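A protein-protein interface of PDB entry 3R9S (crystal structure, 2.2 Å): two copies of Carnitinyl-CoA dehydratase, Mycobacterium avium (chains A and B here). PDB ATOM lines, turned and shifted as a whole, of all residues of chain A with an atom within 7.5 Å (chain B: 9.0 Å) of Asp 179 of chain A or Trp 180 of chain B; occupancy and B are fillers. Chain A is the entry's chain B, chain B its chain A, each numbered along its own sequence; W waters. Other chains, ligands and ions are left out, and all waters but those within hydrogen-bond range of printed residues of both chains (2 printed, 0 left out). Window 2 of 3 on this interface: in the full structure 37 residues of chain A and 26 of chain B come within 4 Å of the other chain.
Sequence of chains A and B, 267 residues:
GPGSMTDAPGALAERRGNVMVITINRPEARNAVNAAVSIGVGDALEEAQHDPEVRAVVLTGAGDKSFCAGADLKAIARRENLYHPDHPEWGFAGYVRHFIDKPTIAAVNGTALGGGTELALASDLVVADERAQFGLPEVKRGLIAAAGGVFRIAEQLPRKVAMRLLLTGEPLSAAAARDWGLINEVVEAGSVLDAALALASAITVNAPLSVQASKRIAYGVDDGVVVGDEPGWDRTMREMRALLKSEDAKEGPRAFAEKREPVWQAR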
ATOM      1  N   LEU A 157     -16.839 -23.877  12.923  1.00  0.00           N
ATOM      2  CA  LEU A 157     -16.223 -22.604  12.574  1.00  0.00           C
ATOM      3  C   LEU A 157     -15.546 -22.056  13.824  1.00  0.00           C
ATOM      4  O   LEU A 157     -15.912 -22.412  14.929  1.00  0.00           O
ATOM      5  CB  LEU A 157     -17.294 -21.602  12.124  1.00  0.00           C
ATOM      6  CG  LEU A 157     -17.667 -21.615  10.642  1.00  0.00           C
ATOM      7  CD1 LEU A 157     -18.812 -20.656  10.396  1.00  0.00           C
ATOM      8  CD2 LEU A 157     -16.447 -21.246   9.768  1.00  0.00           C
ATOM      9  N   SER A 173     -19.930 -17.180   1.780  1.00  0.00           N
ATOM     10  CA  SER A 173     -19.647 -17.766   0.457  1.00  0.00           C
ATOM     11  C   SER A 173     -18.988 -19.144   0.579  1.00  0.00           C
ATOM     12  O   SER A 173     -18.376 -19.454   1.600  1.00  0.00           O
ATOM     13  CB  SER A 173     -18.762 -16.845  -0.376  1.00  0.00           C
ATOM     14  OG  SER A 173     -17.437 -16.792   0.133  1.00  0.00           O
ATOM     15  N   ALA A 174     -19.136 -19.971  -0.450  1.00  0.00           N
ATOM     16  CA  ALA A 174     -18.468 -21.260  -0.479  1.00  0.00           C
ATOM     17  C   ALA A 174     -16.960 -21.066  -0.281  1.00  0.00           C
ATOM     18  O   ALA A 174     -16.340 -21.781   0.507  1.00  0.00           O
ATOM     19  CB  ALA A 174     -18.755 -22.025  -1.804  1.00  0.00           C
ATOM     20  N   ALA A 175     -16.378 -20.101  -0.989  1.00  0.00           N
ATOM     21  CA  ALA A 175     -14.928 -19.832  -0.865  1.00  0.00           C
ATOM     22  C   ALA A 175     -14.509 -19.471   0.583  1.00  0.00           C
ATOM     23  O   ALA A 175     -13.481 -19.945   1.087  1.00  0.00           O
ATOM     24  CB  ALA A 175     -14.491 -18.742  -1.831  1.00  0.00           C
ATOM     25  N   ALA A 176     -15.295 -18.619   1.228  1.00  0.00           N
ATOM     26  CA  ALA A 176     -15.035 -18.219   2.607  1.00  0.00           C
ATOM     27  C   ALA A 176     -15.225 -19.412   3.551  1.00  0.00           C
ATOM     28  O   ALA A 176     -14.436 -19.603   4.457  1.00  0.00           O
ATOM     29  CB  ALA A 176     -15.946 -17.048   3.016  1.00  0.00           C
ATOM     30  N   ALA A 177     -16.268 -20.208   3.339  1.00  0.00           N
ATOM     31  CA  ALA A 177     -16.457 -21.431   4.099  1.00  0.00           C
ATOM     32  C   ALA A 177     -15.216 -22.327   3.989  1.00  0.00           C
ATOM     33  O   ALA A 177     -14.748 -22.883   4.979  1.00  0.00           O
ATOM     34  CB  ALA A 177     -17.688 -22.174   3.622  1.00  0.00           C
ATOM     35  N   ARG A 178     -14.688 -22.451   2.784  1.00  0.00           N
ATOM     36  CA  ARG A 178     -13.504 -23.266   2.556  1.00  0.00           C
ATOM     37  C   ARG A 178     -12.287 -22.646   3.260  1.00  0.00           C
ATOM     38  O   ARG A 178     -11.489 -23.367   3.842  1.00  0.00           O
ATOM     39  CB  ARG A 178     -13.245 -23.424   1.064  1.00  0.00           C
ATOM     40  CG  ARG A 178     -12.419 -24.646   0.659  1.00  0.00           C
ATOM     41  CD  ARG A 178     -10.930 -24.549   0.919  1.00  0.00           C
ATOM     42  NE  ARG A 178     -10.374 -23.187   0.818  1.00  0.00           N
ATOM     43  CZ  ARG A 178      -9.131 -22.861   1.191  1.00  0.00           C
ATOM     44  NH1 ARG A 178      -8.718 -21.601   1.093  1.00  0.00           N
ATOM     45  NH2 ARG A 178      -8.289 -23.788   1.662  1.00  0.00           N
ATOM     46  N   ASP A 179     -12.153 -21.326   3.224  1.00  0.00           N
ATOM     47  CA  ASP A 179     -11.035 -20.651   3.914  1.00  0.00           C
ATOM     48  C   ASP A 179     -11.019 -20.891   5.424  1.00  0.00           C
ATOM     49  O   ASP A 179      -9.955 -21.006   6.029  1.00  0.00           O
ATOM     50  CB  ASP A 179     -11.064 -19.148   3.678  1.00  0.00           C
ATOM     51  CG  ASP A 179     -10.715 -18.775   2.265  1.00  0.00           C
ATOM     52  OD1 ASP A 179     -10.163 -19.641   1.549  1.00  0.00           O
ATOM     53  OD2 ASP A 179     -11.000 -17.616   1.883  1.00  0.00           O
ATOM     54  N   TRP A 180     -12.197 -20.981   6.024  1.00  0.00           N
ATOM     55  CA  TRP A 180     -12.280 -21.235   7.451  1.00  0.00           C
ATOM     56  C   TRP A 180     -12.155 -22.721   7.827  1.00  0.00           C
ATOM     57  O   TRP A 180     -11.991 -23.044   8.994  1.00  0.00           O
ATOM     58  CB  TRP A 180     -13.569 -20.658   8.012  1.00  0.00           C
ATOM     59  CG  TRP A 180     -13.621 -19.190   8.027  1.00  0.00           C
ATOM     60  CD1 TRP A 180     -14.548 -18.401   7.406  1.00  0.00           C
ATOM     61  CD2 TRP A 180     -12.757 -18.303   8.751  1.00  0.00           C
ATOM     62  NE1 TRP A 180     -14.307 -17.070   7.690  1.00  0.00           N
ATOM     63  CE2 TRP A 180     -13.207 -16.984   8.501  1.00  0.00           C
ATOM     64  CE3 TRP A 180     -11.641 -18.491   9.576  1.00  0.00           C
ATOM     65  CZ2 TRP A 180     -12.577 -15.871   9.031  1.00  0.00           C
ATOM     66  CZ3 TRP A 180     -11.013 -17.386  10.098  1.00  0.00           C
ATOM     67  CH2 TRP A 180     -11.490 -16.087   9.839  1.00  0.00           C
ATOM     68  N   GLY A 181     -12.230 -23.612   6.850  1.00  0.00           N
ATOM     69  CA  GLY A 181     -12.195 -25.042   7.112  1.00  0.00           C
ATOM     70  C   GLY A 181     -13.561 -25.651   7.377  1.00  0.00           C
ATOM     71  O   GLY A 181     -13.643 -26.783   7.830  1.00  0.00           O
ATOM     72  N   LEU A 182     -14.638 -24.929   7.084  1.00  0.00           N
ATOM     73  CA  LEU A 182     -15.999 -25.477   7.244  1.00  0.00           C
ATOM     74  C   LEU A 182     -16.363 -26.486   6.164  1.00  0.00           C
ATOM     75  O   LEU A 182     -17.148 -27.403   6.398  1.00  0.00           O
ATOM     76  CB  LEU A 182     -17.036 -24.355   7.220  1.00  0.00           C
ATOM     77  CG  LEU A 182     -18.517 -24.719   7.288  1.00  0.00           C
ATOM     78  CD1 LEU A 182     -18.877 -25.519   8.555  1.00  0.00           C
ATOM     79  CD2 LEU A 182     -19.320 -23.419   7.209  1.00  0.00           C
ATOM     80  N   ILE A 183     -15.826 -26.295   4.966  1.00  0.00           N
ATOM     81  CA  ILE A 183     -16.003 -27.262   3.876  1.00  0.00           C
ATOM     82  C   ILE A 183     -14.623 -27.567   3.293  1.00  0.00           C
ATOM     83  O   ILE A 183     -13.669 -26.817   3.497  1.00  0.00           O
ATOM     84  CB  ILE A 183     -16.973 -26.727   2.784  1.00  0.00           C
ATOM     85  CG1 ILE A 183     -16.357 -25.547   2.022  1.00  0.00           C
ATOM     86  CG2 ILE A 183     -18.324 -26.332   3.407  1.00  0.00           C
ATOM     87  CD1 ILE A 183     -17.029 -25.237   0.684  1.00  0.00           C
ATOM     88  N   ASN A 184     -14.520 -28.658   2.564  1.00  0.00           N
ATOM     89  CA  ASN A 184     -13.229 -29.163   2.124  1.00  0.00           C
ATOM     90  C   ASN A 184     -12.803 -28.687   0.748  1.00  0.00           C
ATOM     91  O   ASN A 184     -11.617 -28.546   0.482  1.00  0.00           O
ATOM     92  CB  ASN A 184     -13.261 -30.688   2.125  1.00  0.00           C
ATOM     93  CG  ASN A 184     -13.570 -31.239   3.478  1.00  0.00           C
ATOM     94  OD1 ASN A 184     -14.724 -31.538   3.778  1.00  0.00           O
ATOM     95  ND2 ASN A 184     -12.556 -31.326   4.338  1.00  0.00           N
ATOM     96  N   VAL A 186     -14.102 -26.481  -3.096  1.00  0.00           N
ATOM     97  CA  VAL A 186     -14.965 -25.612  -3.851  1.00  0.00           C
ATOM     98  C   VAL A 186     -14.664 -25.839  -5.322  1.00  0.00           C
ATOM     99  O   VAL A 186     -13.530 -25.670  -5.757  1.00  0.00           O
ATOM    100  CB  VAL A 186     -14.700 -24.124  -3.497  1.00  0.00           C
ATOM    101  CG1 VAL A 186     -15.424 -23.211  -4.457  1.00  0.00           C
ATOM    102  CG2 VAL A 186     -15.089 -23.829  -2.069  1.00  0.00           C
ATOM    103  N   ILE B 153      -6.994 -34.944  16.430  1.00  0.00           N
ATOM    104  CA  ILE B 153      -6.863 -34.205  15.175  1.00  0.00           C
ATOM    105  C   ILE B 153      -8.028 -33.199  15.017  1.00  0.00           C
ATOM    106  O   ILE B 153      -7.815 -32.055  14.631  1.00  0.00           O
ATOM    107  CB  ILE B 153      -6.658 -35.149  13.965  1.00  0.00           C
ATOM    108  CG1 ILE B 153      -6.134 -34.372  12.752  1.00  0.00           C
ATOM    109  CG2 ILE B 153      -7.940 -35.908  13.620  1.00  0.00           C
ATOM    110  CD1 ILE B 153      -4.707 -33.921  12.863  1.00  0.00           C
ATOM    111  N   GLU B 155      -9.662 -31.856  17.479  1.00  0.00           N
ATOM    112  CA  GLU B 155      -9.530 -30.823  18.506  1.00  0.00           C
ATOM    113  C   GLU B 155      -8.573 -29.721  18.064  1.00  0.00           C
ATOM    114  O   GLU B 155      -8.645 -28.604  18.555  1.00  0.00           O
ATOM    115  CB  GLU B 155      -9.031 -31.412  19.827  1.00  0.00           C
ATOM    116  CG  GLU B 155     -10.100 -32.162  20.587  1.00  0.00           C
ATOM    117  CD  GLU B 155      -9.571 -33.194  21.594  1.00  0.00           C
ATOM    118  OE1 GLU B 155      -8.332 -33.344  21.754  1.00  0.00           O
ATOM    119  OE2 GLU B 155     -10.423 -33.877  22.214  1.00  0.00           O
ATOM    120  N   GLN B 156      -7.674 -30.043  17.144  1.00  0.00           N
ATOM    121  CA  GLN B 156      -6.591 -29.153  16.778  1.00  0.00           C
ATOM    122  C   GLN B 156      -6.661 -28.631  15.330  1.00  0.00           C
ATOM    123  O   GLN B 156      -5.856 -27.781  14.936  1.00  0.00           O
ATOM    124  CB  GLN B 156      -5.255 -29.863  17.049  1.00  0.00           C
ATOM    125  CG  GLN B 156      -5.115 -30.356  18.510  1.00  0.00           C
ATOM    126  CD  GLN B 156      -3.695 -30.780  18.873  1.00  0.00           C
ATOM    127  OE1 GLN B 156      -2.734 -30.424  18.181  1.00  0.00           O
ATOM    128  NE2 GLN B 156      -3.553 -31.526  19.973  1.00  0.00           N
ATOM    129  N   LEU B 157      -7.604 -29.143  14.543  1.00  0.00           N
ATOM    130  CA  LEU B 157      -7.865 -28.644  13.189  1.00  0.00           C
ATOM    131  C   LEU B 157      -9.339 -28.458  13.059  1.00  0.00           C
ATOM    132  O   LEU B 157     -10.094 -29.081  13.785  1.00  0.00           O
ATOM    133  CB  LEU B 157      -7.453 -29.659  12.138  1.00  0.00           C
ATOM    134  CG  LEU B 157      -6.000 -29.706  11.691  1.00  0.00           C
ATOM    135  CD1 LEU B 157      -5.761 -30.990  10.881  1.00  0.00           C
ATOM    136  CD2 LEU B 157      -5.678 -28.468  10.873  1.00  0.00           C
ATOM    137  N   PRO B 158      -9.777 -27.611  12.118  1.00  0.00           N
ATOM    138  CA  PRO B 158     -11.231 -27.538  11.922  1.00  0.00           C
ATOM    139  C   PRO B 158     -11.823 -28.909  11.584  1.00  0.00           C
ATOM    140  O   PRO B 158     -11.178 -29.729  10.918  1.00  0.00           O
ATOM    141  CB  PRO B 158     -11.370 -26.567  10.750  1.00  0.00           C
ATOM    142  CG  PRO B 158     -10.136 -25.727  10.803  1.00  0.00           C
ATOM    143  CD  PRO B 158      -9.061 -26.696  11.211  1.00  0.00           C
ATOM    144  N   ARG B 159     -13.035 -29.145  12.065  1.00  0.00           N
ATOM    145  CA  ARG B 159     -13.683 -30.453  11.972  1.00  0.00           C
ATOM    146  C   ARG B 159     -13.568 -31.087  10.589  1.00  0.00           C
ATOM    147  O   ARG B 159     -13.099 -32.236  10.459  1.00  0.00           O
ATOM    148  CB  ARG B 159     -15.146 -30.306  12.388  1.00  0.00           C
ATOM    149  CG  ARG B 159     -16.095 -31.447  12.056  1.00  0.00           C
ATOM    150  CD  ARG B 159     -15.755 -32.721  12.777  1.00  0.00           C
ATOM    151  NE  ARG B 159     -15.917 -32.647  14.230  1.00  0.00           N
ATOM    152  CZ  ARG B 159     -15.554 -33.632  15.068  1.00  0.00           C
ATOM    153  NH1 ARG B 159     -15.720 -33.494  16.377  1.00  0.00           N
ATOM    154  NH2 ARG B 159     -15.002 -34.760  14.604  1.00  0.00           N
ATOM    155  N   LYS B 160     -13.984 -30.354   9.561  1.00  0.00           N
ATOM    156  CA  LYS B 160     -13.976 -30.923   8.207  1.00  0.00           C
ATOM    157  C   LYS B 160     -12.557 -31.224   7.703  1.00  0.00           C
ATOM    158  O   LYS B 160     -12.358 -32.227   7.056  1.00  0.00           O
ATOM    159  CB  LYS B 160     -14.691 -30.004   7.213  1.00  0.00           C
ATOM    160  CG  LYS B 160     -16.096 -30.468   6.791  1.00  0.00           C
ATOM    161  CD  LYS B 160     -17.105 -30.382   7.898  1.00  0.00           C
ATOM    162  CE  LYS B 160     -18.464 -30.964   7.483  1.00  0.00           C
ATOM    163  NZ  LYS B 160     -19.311 -31.139   8.683  1.00  0.00           N
ATOM    164  N   VAL B 161     -11.604 -30.335   7.985  1.00  0.00           N
ATOM    165  CA  VAL B 161     -10.215 -30.501   7.580  1.00  0.00           C
ATOM    166  C   VAL B 161      -9.616 -31.700   8.315  1.00  0.00           C
ATOM    167  O   VAL B 161      -8.939 -32.538   7.693  1.00  0.00           O
ATOM    168  CB  VAL B 161      -9.356 -29.231   7.864  1.00  0.00           C
ATOM    169  CG1 VAL B 161      -7.916 -29.433   7.391  1.00  0.00           C
ATOM    170  CG2 VAL B 161      -9.983 -27.954   7.193  1.00  0.00           C
ATOM    171  N   ALA B 162      -9.891 -31.797   9.625  1.00  0.00           N
ATOM    172  CA  ALA B 162      -9.465 -32.947  10.412  1.00  0.00           C
ATOM    173  C   ALA B 162     -10.027 -34.260   9.870  1.00  0.00           C
ATOM    174  O   ALA B 162      -9.309 -35.241   9.782  1.00  0.00           O
ATOM    175  CB  ALA B 162      -9.861 -32.779  11.901  1.00  0.00           C
ATOM    176  N   ARG B 164     -11.117 -35.117   6.788  1.00  0.00           N
ATOM    177  CA  ARG B 164     -10.483 -35.448   5.505  1.00  0.00           C
ATOM    178  C   ARG B 164      -9.141 -36.158   5.742  1.00  0.00           C
ATOM    179  O   ARG B 164      -8.855 -37.208   5.162  1.00  0.00           O
ATOM    180  CB  ARG B 164     -10.255 -34.167   4.702  1.00  0.00           C
ATOM    181  CG  ARG B 164      -9.551 -34.343   3.358  1.00  0.00           C
ATOM    182  CD  ARG B 164      -9.445 -32.997   2.621  1.00  0.00           C
ATOM    183  NE  ARG B 164      -9.610 -33.146   1.181  1.00  0.00           N
ATOM    184  CZ  ARG B 164      -9.828 -32.145   0.322  1.00  0.00           C
ATOM    185  NH1 ARG B 164      -9.983 -32.431  -0.956  1.00  0.00           N
ATOM    186  NH2 ARG B 164      -9.893 -30.872   0.722  1.00  0.00           N
ATOM    187  N   LEU B 165      -8.321 -35.543   6.593  1.00  0.00           N
ATOM    188  CA  LEU B 165      -6.989 -36.053   6.897  1.00  0.00           C
ATOM    189  C   LEU B 165      -7.094 -37.462   7.489  1.00  0.00           C
ATOM    190  O   LEU B 165      -6.409 -38.404   7.060  1.00  0.00           O
ATOM    191  CB  LEU B 165      -6.303 -35.080   7.856  1.00  0.00           C
ATOM    192  CG  LEU B 165      -4.820 -35.205   8.178  1.00  0.00           C
ATOM    193  CD1 LEU B 165      -4.284 -33.839   8.639  1.00  0.00           C
ATOM    194  CD2 LEU B 165      -4.604 -36.257   9.233  1.00  0.00           C
ATOM    195  N   LEU B 172      -0.084 -33.820   4.648  1.00  0.00           N
ATOM    196  CA  LEU B 172      -0.292 -32.371   4.734  1.00  0.00           C
ATOM    197  C   LEU B 172       1.078 -31.743   4.843  1.00  0.00           C
ATOM    198  O   LEU B 172       1.862 -32.130   5.715  1.00  0.00           O
ATOM    199  CB  LEU B 172      -1.110 -32.070   6.005  1.00  0.00           C
ATOM    200  CG  LEU B 172      -1.605 -30.677   6.327  1.00  0.00           C
ATOM    201  CD1 LEU B 172      -2.822 -30.316   5.500  1.00  0.00           C
ATOM    202  CD2 LEU B 172      -1.933 -30.631   7.794  1.00  0.00           C
ATOM    203  N   SER B 173       1.386 -30.775   3.986  1.00  0.00           N
ATOM    204  CA  SER B 173       2.690 -30.093   4.042  1.00  0.00           C
ATOM    205  C   SER B 173       2.837 -29.275   5.337  1.00  0.00           C
ATOM    206  O   SER B 173       1.842 -28.918   5.975  1.00  0.00           O
ATOM    207  CB  SER B 173       2.864 -29.164   2.840  1.00  0.00           C
ATOM    208  OG  SER B 173       2.096 -27.971   3.003  1.00  0.00           O
ATOM    209  N   ALA B 174       4.077 -28.977   5.717  1.00  0.00           N
ATOM    210  CA  ALA B 174       4.325 -28.152   6.878  1.00  0.00           C
ATOM    211  C   ALA B 174       3.645 -26.764   6.706  1.00  0.00           C
ATOM    212  O   ALA B 174       3.053 -26.238   7.644  1.00  0.00           O
ATOM    213  CB  ALA B 174       5.808 -28.015   7.122  1.00  0.00           C
ATOM    214  N   ALA B 175       3.685 -26.224   5.494  1.00  0.00           N
ATOM    215  CA  ALA B 175       3.100 -24.911   5.206  1.00  0.00           C
ATOM    216  C   ALA B 175       1.589 -24.920   5.413  1.00  0.00           C
ATOM    217  O   ALA B 175       1.036 -24.002   6.020  1.00  0.00           O
ATOM    218  CB  ALA B 175       3.449 -24.463   3.768  1.00  0.00           C
ATOM    219  N   ALA B 176       0.928 -25.970   4.924  1.00  0.00           N
ATOM    220  CA  ALA B 176      -0.513 -26.084   5.096  1.00  0.00           C
ATOM    221  C   ALA B 176      -0.839 -26.329   6.575  1.00  0.00           C
ATOM    222  O   ALA B 176      -1.764 -25.733   7.120  1.00  0.00           O
ATOM    223  CB  ALA B 176      -1.117 -27.174   4.173  1.00  0.00           C
ATOM    224  N   ALA B 177      -0.059 -27.163   7.245  1.00  0.00           N
ATOM    225  CA  ALA B 177      -0.235 -27.339   8.691  1.00  0.00           C
ATOM    226  C   ALA B 177      -0.209 -25.990   9.430  1.00  0.00           C
ATOM    227  O   ALA B 177      -1.073 -25.715  10.283  1.00  0.00           O
ATOM    228  CB  ALA B 177       0.821 -28.270   9.257  1.00  0.00           C
ATOM    229  N   ARG B 178       0.790 -25.171   9.110  1.00  0.00           N
ATOM    230  CA  ARG B 178       0.968 -23.863   9.737  1.00  0.00           C
ATOM    231  C   ARG B 178      -0.177 -22.930   9.384  1.00  0.00           C
ATOM    232  O   ARG B 178      -0.686 -22.246  10.257  1.00  0.00           O
ATOM    233  CB  ARG B 178       2.316 -23.248   9.322  1.00  0.00           C
ATOM    234  CG  ARG B 178       2.614 -21.861   9.915  1.00  0.00           C
ATOM    235  CD  ARG B 178       2.170 -20.682   9.010  1.00  0.00           C
ATOM    236  NE  ARG B 178       2.099 -21.003   7.572  1.00  0.00           N
ATOM    237  CZ  ARG B 178       3.064 -20.788   6.666  1.00  0.00           C
ATOM    238  NH1 ARG B 178       4.235 -20.237   7.006  1.00  0.00           N
ATOM    239  NH2 ARG B 178       2.856 -21.126   5.397  1.00  0.00           N
ATOM    240  N   ASP B 179      -0.588 -22.923   8.113  1.00  0.00           N
ATOM    241  CA  ASP B 179      -1.731 -22.106   7.658  1.00  0.00           C
ATOM    242  C   ASP B 179      -3.031 -22.425   8.408  1.00  0.00           C
ATOM    243  O   ASP B 179      -3.866 -21.534   8.632  1.00  0.00           O
ATOM    244  CB  ASP B 179      -1.993 -22.296   6.153  1.00  0.00           C
ATOM    245  CG  ASP B 179      -1.006 -21.561   5.293  1.00  0.00           C
ATOM    246  OD1 ASP B 179      -0.105 -20.873   5.845  1.00  0.00           O
ATOM    247  OD2 ASP B 179      -1.134 -21.674   4.052  1.00  0.00           O
ATOM    248  N   TRP B 180      -3.216 -23.695   8.739  1.00  0.00           N
ATOM    249  CA  TRP B 180      -4.393 -24.130   9.491  1.00  0.00           C
ATOM    250  C   TRP B 180      -4.286 -23.896  10.996  1.00  0.00           C
ATOM    251  O   TRP B 180      -5.291 -23.977  11.705  1.00  0.00           O
ATOM    252  CB  TRP B 180      -4.669 -25.607   9.244  1.00  0.00           C
ATOM    253  CG  TRP B 180      -5.296 -25.881   7.924  1.00  0.00           C
ATOM    254  CD1 TRP B 180      -4.822 -26.703   6.950  1.00  0.00           C
ATOM    255  CD2 TRP B 180      -6.529 -25.335   7.427  1.00  0.00           C
ATOM    256  NE1 TRP B 180      -5.685 -26.710   5.881  1.00  0.00           N
ATOM    257  CE2 TRP B 180      -6.735 -25.875   6.143  1.00  0.00           C
ATOM    258  CE3 TRP B 180      -7.478 -24.452   7.946  1.00  0.00           C
ATOM    259  CZ2 TRP B 180      -7.849 -25.554   5.361  1.00  0.00           C
ATOM    260  CZ3 TRP B 180      -8.577 -24.133   7.176  1.00  0.00           C
ATOM    261  CH2 TRP B 180      -8.753 -24.679   5.890  1.00  0.00           C
ATOM    262  N   GLY B 181      -3.083 -23.607  11.486  1.00  0.00           N
ATOM    263  CA  GLY B 181      -2.883 -23.412  12.921  1.00  0.00           C
ATOM    264  C   GLY B 181      -2.665 -24.701  13.684  1.00  0.00           C
ATOM    265  O   GLY B 181      -2.700 -24.697  14.911  1.00  0.00           O
ATOM    266  N   LEU B 182      -2.460 -25.804  12.962  1.00  0.00           N
ATOM    267  CA  LEU B 182      -2.015 -27.074  13.544  1.00  0.00           C
ATOM    268  C   LEU B 182      -0.587 -27.000  14.087  1.00  0.00           C
ATOM    269  O   LEU B 182      -0.267 -27.656  15.075  1.00  0.00           O
ATOM    270  CB  LEU B 182      -2.060 -28.186  12.496  1.00  0.00           C
ATOM    271  CG  LEU B 182      -1.613 -29.575  12.973  1.00  0.00           C
ATOM    272  CD1 LEU B 182      -2.469 -30.044  14.147  1.00  0.00           C
ATOM    273  CD2 LEU B 182      -1.668 -30.563  11.839  1.00  0.00           C
ATOM    274  N   ILE B 183       0.283 -26.259  13.412  1.00  0.00           N
ATOM    275  CA  ILE B 183       1.619 -25.995  13.951  1.00  0.00           C
ATOM    276  C   ILE B 183       1.865 -24.503  14.064  1.00  0.00           C
ATOM    277  O   ILE B 183       1.157 -23.694  13.454  1.00  0.00           O
ATOM    278  CB  ILE B 183       2.717 -26.683  13.134  1.00  0.00           C
ATOM    279  CG1 ILE B 183       2.843 -26.041  11.749  1.00  0.00           C
ATOM    280  CG2 ILE B 183       2.418 -28.200  13.046  1.00  0.00           C
ATOM    281  CD1 ILE B 183       4.143 -26.340  11.076  1.00  0.00           C
ATOM    282  N   ASN B 184       2.876 -24.147  14.839  1.00  0.00           N
ATOM    283  CA  ASN B 184       3.182 -22.745  15.150  1.00  0.00           C
ATOM    284  C   ASN B 184       4.048 -22.022  14.137  1.00  0.00           C
ATOM    285  O   ASN B 184       3.822 -20.846  13.832  1.00  0.00           O
ATOM    286  CB  ASN B 184       3.845 -22.687  16.498  1.00  0.00           C
ATOM    287  CG  ASN B 184       2.937 -23.160  17.570  1.00  0.00           C
ATOM    288  OD1 ASN B 184       3.047 -24.300  18.026  1.00  0.00           O
ATOM    289  ND2 ASN B 184       1.983 -22.301  17.959  1.00  0.00           N
ATOM    290  N   VAL B 186       6.916 -22.553  10.527  1.00  0.00           N
ATOM    291  CA  VAL B 186       7.666 -23.231   9.491  1.00  0.00           C
ATOM    292  C   VAL B 186       8.951 -22.455   9.286  1.00  0.00           C
ATOM    293  O   VAL B 186       8.920 -21.235   9.174  1.00  0.00           O
ATOM    294  CB  VAL B 186       6.855 -23.288   8.191  1.00  0.00           C
ATOM    295  CG1 VAL B 186       7.683 -23.868   7.031  1.00  0.00           C
ATOM    296  CG2 VAL B 186       5.623 -24.134   8.429  1.00  0.00           C
HETATM  297  O   HOH W   1      -9.779 -30.276   3.503  1.00  0.00           O
HETATM  298  O   HOH W   2     -15.072 -27.600  10.087  1.00  0.00           O
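Water W2 lies within hydrogen-bond range of O of Gly 181 of chain A (2.8 Å), N of Lys 160 of chain B (3.0 Å) and N of Arg 159 of chain B (3.2 Å).
Water W1 bridges NH2 of Arg 164 of chain B and ND2 of Asn 184 of chain A.
Ser 173 of chain A touches none of the printed residues of chain B.
Arg 178 of chain A touches one residue of chain B.
Of chain B, only Trp 180 comes within 4 Å of Asp 179 of chain A.
Of the printed residues of chain B, Gly 181 of chain A touches Pro 158, Lys 160, Val 161 and Trp 180.
Printed residues of chain B within 4 Å of Asn 184 of chain A: Lys 160 (2.9 Å), Val 161 (3.9 Å) and Arg 164 (2.9 Å).
Of the printed residues of chain A, Pro 158 of chain B touches Trp 180 (3.7 Å) and Gly 181 (3.7 Å).
Of the printed residues of chain A, Val 161 of chain B touches Gly 181 (3.7 Å) and Asn 184 (3.9 Å).
Printed residues of chain A within 4 Å of Arg 164 of chain B: Asn 184.
Trp 180 of chain B touches just these residues of chain A: Arg 178 (3.7 Å), Asp 179 (3.6 Å), Trp 180 (3.9 Å) and Gly 181 (3.7 Å).
The nearest residue of chain B that does not touch Asp 179 of chain A is Asp 179 of chain B (6.6 Å).
The nearest residue of chain A that does not touch Trp 180 of chain B is Ile 183 of chain A (5.9 Å).
The nearest printed residue of chain A that does not touch Pro 158 of chain B is Leu 182 of chain A (5.2 Å).
ND2 of Asn 184 of chain A is in hydrogen-bond range of O of Lys 160 of chain B, at 2.9 Å.
The backbone carbonyl oxygen (O) of Asn 184 of chain A sits at hydrogen-bond distance from the guanidinium group (NH2) of Arg 164 of chain B, at 2.9 Å.
Among the printed residues, merely in contact across the chains: Arg 178 of chain A with Trp 180 of chain B (3.7 Å), Asp 179 of chain A with Trp 180 of chain B (3.6 Å), Trp 180 of chain A with Pro 158 of chain B (3.7 Å), Trp 180 of chain A with Trp 180 of chain B (3.9 Å), Gly 181 of chain A with Pro 158 of chain B (3.7 Å), Gly 181 of chain A with Lys 160 of chain B (3.4 Å), Gly 181 of chain A with Val 161 of chain B (3.7 Å), Gly 181 of chain A with Trp 180 of chain B (3.7 Å), Leu 182 of chain A with Lys 160 of chain B (3.3 Å) and Asn 184 of chain A with Val 161 of chain B (3.9 Å).
Arg 178 of chain A touches Trp 180 of chain B, but with the chains exchanged Trp 180 of chain A does not touch Arg 178 of chain B (11.4 Å).
Trp 180 of chain B touches its own counterpart, Trp 180 of chain A.
Gly 181 of chain A touches Trp 180 of chain B, but with the chains exchanged Trp 180 of chain A does not touch Gly 181 of chain B (9.3 Å).
14 positions are printed for both chains.
Of the 12 pairs that touch across the chains among the printed residues, 1 has its exchanged pair printed and touching as well.
The backbone NH (N) of Leu 182 of chain A sits at hydrogen-bond distance from the backbone carbonyl oxygen (O) of Ala 177 of chain A (2.9 Å).
The guanidinium group (NH1) of Arg 178 of chain A lies within salt-bridge range of the side-chain carboxylate (OD1) of Asp 179 of chain A, 2.5 Å away.
Of the 14 printed residues of chain A, 6 touch a printed residue of chain B.
Of the 25 printed residues of chain B, 5 touch a printed residue of chain A.
Hydrophobic or aromatic side chains of chain B within 4 Å of the printed part of chain A: Pro 158, Val 161 and Trp 180.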
